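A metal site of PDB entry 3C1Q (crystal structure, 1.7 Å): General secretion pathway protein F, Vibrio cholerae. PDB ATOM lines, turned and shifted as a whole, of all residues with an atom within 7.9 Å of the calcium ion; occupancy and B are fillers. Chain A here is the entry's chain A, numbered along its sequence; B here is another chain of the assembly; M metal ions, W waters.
The calcium ion is bound by OE2 of Glu 97, at 2.3 Å.
OE2 of Glu 43 of chain B binds the calcium ion (2.3 Å).
The calcium ion is bound by water W2.
The calcium ion is bound by water W3.
Water W1 binds the calcium ion, at 2.4 Å.
The calcium ion is bound by OD2 of Asp 101 (2.5 Å).
The calcium ion is bound by OD1 of Asp 101 (2.5 Å).
Of the 16 residues printed, 3 come within 4 Å of the calcium ion.
OE1 of Glu 97 lies within salt-bridge range of NH1 of Arg 19, 3.4 Å away.
OE1 of Glu 97 is in hydrogen-bond range of NE2 of Gln 26, 2.8 Å away.
OD1 of Asp 101 sits close to NH2 of Arg 19 (2.8 Å).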
ATOM      1  N   ARG A  19       5.387  13.941  -7.615  1.00  0.00           N
ATOM      2  CA  ARG A  19       6.536  13.583  -6.783  1.00  0.00           C
ATOM      3  C   ARG A  19       6.295  13.959  -5.306  1.00  0.00           C
ATOM      4  O   ARG A  19       6.518  13.152  -4.402  1.00  0.00           O
ATOM      5  CB  ARG A  19       7.824  14.223  -7.332  1.00  0.00           C
ATOM      6  CG  ARG A  19       9.039  14.015  -6.452  1.00  0.00           C
ATOM      7  CD  ARG A  19       9.373  12.533  -6.269  1.00  0.00           C
ATOM      8  NE  ARG A  19       9.730  11.945  -7.562  1.00  0.00           N
ATOM      9  CZ  ARG A  19       9.773  10.639  -7.780  1.00  0.00           C
ATOM     10  NH1 ARG A  19       9.504   9.788  -6.822  1.00  0.00           N
ATOM     11  NH2 ARG A  19      10.117  10.175  -8.994  1.00  0.00           N
ATOM     12  N   GLN A  26       4.117   8.076   0.902  1.00  0.00           N
ATOM     13  CA  GLN A  26       5.007   6.974   1.255  1.00  0.00           C
ATOM     14  C   GLN A  26       5.618   7.134   2.639  1.00  0.00           C
ATOM     15  O   GLN A  26       5.972   6.149   3.270  1.00  0.00           O
ATOM     16  CB  GLN A  26       6.090   6.803   0.195  1.00  0.00           C
ATOM     17  CG  GLN A  26       5.532   6.096  -1.047  1.00  0.00           C
ATOM     18  CD  GLN A  26       6.542   5.921  -2.144  1.00  0.00           C
ATOM     19  OE1 GLN A  26       7.100   4.835  -2.327  1.00  0.00           O
ATOM     20  NE2 GLN A  26       6.777   6.964  -2.904  1.00  0.00           N
ATOM     21  N   SER A  94       2.970   2.644  -3.696  1.00  0.00           N
ATOM     22  CA  SER A  94       3.850   2.248  -4.794  1.00  0.00           C
ATOM     23  C   SER A  94       3.331   2.683  -6.169  1.00  0.00           C
ATOM     24  O   SER A  94       4.144   2.932  -7.071  1.00  0.00           O
ATOM     25  CB  SER A  94       4.172   0.753  -4.753  1.00  0.00           C
ATOM     26  OG  SER A  94       3.027  -0.050  -4.877  1.00  0.00           O
ATOM     27  N   LEU A  96       1.694   5.577  -6.555  1.00  0.00           N
ATOM     28  CA  LEU A  96       2.066   7.014  -6.581  1.00  0.00           C
ATOM     29  C   LEU A  96       3.548   7.184  -6.974  1.00  0.00           C
ATOM     30  O   LEU A  96       3.871   8.033  -7.795  1.00  0.00           O
ATOM     31  CB  LEU A  96       1.760   7.716  -5.251  1.00  0.00           C
ATOM     32  CG  LEU A  96       0.278   8.038  -4.999  1.00  0.00           C
ATOM     33  CD1 LEU A  96       0.132   8.645  -3.610  1.00  0.00           C
ATOM     34  CD2 LEU A  96      -0.309   8.977  -6.040  1.00  0.00           C
ATOM     35  N   GLU A  97       4.415   6.329  -6.437  1.00  0.00           N
ATOM     36  CA  GLU A  97       5.822   6.315  -6.867  1.00  0.00           C
ATOM     37  C   GLU A  97       5.954   6.126  -8.366  1.00  0.00           C
ATOM     38  O   GLU A  97       6.696   6.828  -9.039  1.00  0.00           O
ATOM     39  CB  GLU A  97       6.596   5.221  -6.129  1.00  0.00           C
ATOM     40  CG  GLU A  97       8.067   5.174  -6.474  1.00  0.00           C
ATOM     41  CD  GLU A  97       8.803   6.445  -6.174  1.00  0.00           C
ATOM     42  OE1 GLU A  97       8.535   7.059  -5.113  1.00  0.00           O
ATOM     43  OE2 GLU A  97       9.683   6.840  -6.990  1.00  0.00           O
ATOM     44  N   ARG A  98       5.235   5.142  -8.884  1.00  0.00           N
ATOM     45  CA  ARG A  98       5.231   4.873 -10.299  1.00  0.00           C
ATOM     46  C   ARG A  98       4.747   6.082 -11.099  1.00  0.00           C
ATOM     47  O   ARG A  98       5.360   6.471 -12.114  1.00  0.00           O
ATOM     48  CB  ARG A  98       4.332   3.699 -10.537  1.00  0.00           C
ATOM     49  CG  ARG A  98       4.322   3.212 -11.842  1.00  0.00           C
ATOM     50  CD  ARG A  98       5.600   2.458 -12.214  1.00  0.00           C
ATOM     51  NE  ARG A  98       5.252   2.086 -13.540  1.00  0.00           N
ATOM     52  CZ  ARG A  98       4.699   0.936 -13.901  1.00  0.00           C
ATOM     53  NH1 ARG A  98       4.587  -0.087 -13.071  1.00  0.00           N
ATOM     54  NH2 ARG A  98       4.343   0.835 -15.154  1.00  0.00           N
ATOM     55  N   ALA A 100       4.852   9.186 -10.162  1.00  0.00           N
ATOM     56  CA  ALA A 100       5.882  10.239 -10.045  1.00  0.00           C
ATOM     57  C   ALA A 100       7.019  10.021 -11.033  1.00  0.00           C
ATOM     58  O   ALA A 100       7.480  10.950 -11.721  1.00  0.00           O
ATOM     59  CB  ALA A 100       6.427  10.305  -8.612  1.00  0.00           C
ATOM     60  N   ASP A 101       7.503   8.783 -11.094  1.00  0.00           N
ATOM     61  CA  ASP A 101       8.529   8.416 -12.053  1.00  0.00           C
ATOM     62  C   ASP A 101       8.034   8.692 -13.484  1.00  0.00           C
ATOM     63  O   ASP A 101       8.763   9.233 -14.322  1.00  0.00           O
ATOM     64  CB  ASP A 101       8.927   6.951 -11.923  1.00  0.00           C
ATOM     65  CG  ASP A 101       9.733   6.654 -10.674  1.00  0.00           C
ATOM     66  OD1 ASP A 101      10.355   7.579 -10.107  1.00  0.00           O
ATOM     67  OD2 ASP A 101       9.778   5.479 -10.283  1.00  0.00           O
ATOM     68  N   TYR A 102       6.776   8.320 -13.744  1.00  0.00           N
ATOM     69  CA  TYR A 102       6.141   8.519 -15.060  1.00  0.00           C
ATOM     70  C   TYR A 102       6.069   9.996 -15.413  1.00  0.00           C
ATOM     71  O   TYR A 102       6.488  10.396 -16.502  1.00  0.00           O
ATOM     72  CB  TYR A 102       4.747   7.878 -15.086  1.00  0.00           C
ATOM     73  CG  TYR A 102       3.752   8.495 -16.051  1.00  0.00           C
ATOM     74  CD1 TYR A 102       3.768   8.186 -17.409  1.00  0.00           C
ATOM     75  CD2 TYR A 102       2.774   9.388 -15.604  1.00  0.00           C
ATOM     76  CE1 TYR A 102       2.850   8.772 -18.307  1.00  0.00           C
ATOM     77  CE2 TYR A 102       1.862   9.962 -16.473  1.00  0.00           C
ATOM     78  CZ  TYR A 102       1.893   9.662 -17.810  1.00  0.00           C
ATOM     79  OH  TYR A 102       0.951  10.255 -18.638  1.00  0.00           O
ATOM     80  N   GLU A 104       7.813  12.488 -14.249  1.00  0.00           N
ATOM     81  CA  GLU A 104       9.155  13.060 -14.414  1.00  0.00           C
ATOM     82  C   GLU A 104       9.750  12.665 -15.774  1.00  0.00           C
ATOM     83  O   GLU A 104      10.385  13.472 -16.466  1.00  0.00           O
ATOM     84  CB  GLU A 104      10.046  12.619 -13.261  1.00  0.00           C
ATOM     85  CG  GLU A 104       9.750  13.351 -11.996  1.00  0.00           C
ATOM     86  CD  GLU A 104      10.566  12.879 -10.803  1.00  0.00           C
ATOM     87  OE1 GLU A 104      11.329  11.895 -10.956  1.00  0.00           O
ATOM     88  OE2 GLU A 104      10.424  13.517  -9.723  1.00  0.00           O
ATOM     89  N   LEU B  16      16.089  15.857  -6.765  1.00  0.00           N
ATOM     90  CA  LEU B  16      15.074  14.969  -6.261  1.00  0.00           C
ATOM     91  C   LEU B  16      15.158  14.931  -4.736  1.00  0.00           C
ATOM     92  O   LEU B  16      14.164  15.228  -4.057  1.00  0.00           O
ATOM     93  CB  LEU B  16      15.261  13.569  -6.840  1.00  0.00           C
ATOM     94  CG  LEU B  16      14.419  12.430  -6.260  1.00  0.00           C
ATOM     95  CD1 LEU B  16      12.927  12.732  -6.416  1.00  0.00           C
ATOM     96  CD2 LEU B  16      14.787  11.109  -6.911  1.00  0.00           C
ATOM     97  N   GLN B  20      12.400  16.396  -2.055  1.00  0.00           N
ATOM     98  CA  GLN B  20      11.744  15.470  -1.135  1.00  0.00           C
ATOM     99  C   GLN B  20      11.987  15.883   0.315  1.00  0.00           C
ATOM    100  O   GLN B  20      11.054  15.942   1.117  1.00  0.00           O
ATOM    101  CB  GLN B  20      12.210  14.038  -1.363  1.00  0.00           C
ATOM    102  CG  GLN B  20      11.832  13.477  -2.729  1.00  0.00           C
ATOM    103  CD  GLN B  20      12.329  12.071  -2.934  1.00  0.00           C
ATOM    104  OE1 GLN B  20      13.525  11.812  -2.865  1.00  0.00           O
ATOM    105  NE2 GLN B  20      11.390  11.141  -3.176  1.00  0.00           N
ATOM    106  N   GLN B  41      12.816   5.756  -0.164  1.00  0.00           N
ATOM    107  CA  GLN B  41      12.265   6.017  -1.494  1.00  0.00           C
ATOM    108  C   GLN B  41      13.306   6.111  -2.620  1.00  0.00           C
ATOM    109  O   GLN B  41      12.951   6.300  -3.769  1.00  0.00           O
ATOM    110  CB  GLN B  41      11.397   7.285  -1.451  1.00  0.00           C
ATOM    111  CG  GLN B  41      10.175   7.137  -0.548  1.00  0.00           C
ATOM    112  CD  GLN B  41       9.405   8.419  -0.398  1.00  0.00           C
ATOM    113  OE1 GLN B  41       9.345   9.229  -1.330  1.00  0.00           O
ATOM    114  NE2 GLN B  41       8.822   8.636   0.784  1.00  0.00           N
ATOM    115  N   SER B  42      14.578   5.958  -2.299  1.00  0.00           N
ATOM    116  CA  SER B  42      15.632   6.163  -3.303  1.00  0.00           C
ATOM    117  C   SER B  42      15.828   4.932  -4.176  1.00  0.00           C
ATOM    118  O   SER B  42      15.878   3.842  -3.650  1.00  0.00           O
ATOM    119  CB  SER B  42      16.969   6.502  -2.629  1.00  0.00           C
ATOM    120  OG  SER B  42      17.904   6.917  -3.621  1.00  0.00           O
ATOM    121  N   GLU B  43      15.983   5.130  -5.489  1.00  0.00           N
ATOM    122  CA  GLU B  43      16.291   4.068  -6.447  1.00  0.00           C
ATOM    123  C   GLU B  43      17.770   3.750  -6.487  1.00  0.00           C
ATOM    124  O   GLU B  43      18.160   2.686  -6.962  1.00  0.00           O
ATOM    125  CB  GLU B  43      15.920   4.479  -7.885  1.00  0.00           C
ATOM    126  CG  GLU B  43      14.527   4.931  -8.090  1.00  0.00           C
ATOM    127  CD  GLU B  43      14.189   5.234  -9.545  1.00  0.00           C
ATOM    128  OE1 GLU B  43      15.045   5.055 -10.437  1.00  0.00           O
ATOM    129  OE2 GLU B  43      13.044   5.649  -9.787  1.00  0.00           O
ATOM    130  N   LYS B  44      18.594   4.696  -6.040  1.00  0.00           N
ATOM    131  CA  LYS B  44      20.042   4.654  -6.185  1.00  0.00           C
ATOM    132  C   LYS B  44      20.669   4.155  -4.871  1.00  0.00           C
ATOM    133  O   LYS B  44      20.664   4.860  -3.872  1.00  0.00           O
ATOM    134  CB  LYS B  44      20.542   6.056  -6.501  1.00  0.00           C
ATOM    135  CG  LYS B  44      20.020   6.666  -7.826  1.00  0.00           C
ATOM    136  CD  LYS B  44      20.746   6.046  -9.016  1.00  0.00           C
ATOM    137  CE  LYS B  44      20.882   7.006 -10.196  1.00  0.00           C
ATOM    138  NZ  LYS B  44      19.590   7.598 -10.586  1.00  0.00           N
HETATM  139 CA    CA M   1      11.285   5.999  -8.344  1.00  0.00          CA
HETATM  140  O   HOH W   1      12.540   7.971  -7.691  1.00  0.00           O
HETATM  141  O   HOH W   2      12.114   5.188  -6.318  1.00  0.00           O
HETATM  142  O   HOH W   3      10.897   3.655  -8.294  1.00  0.00           O
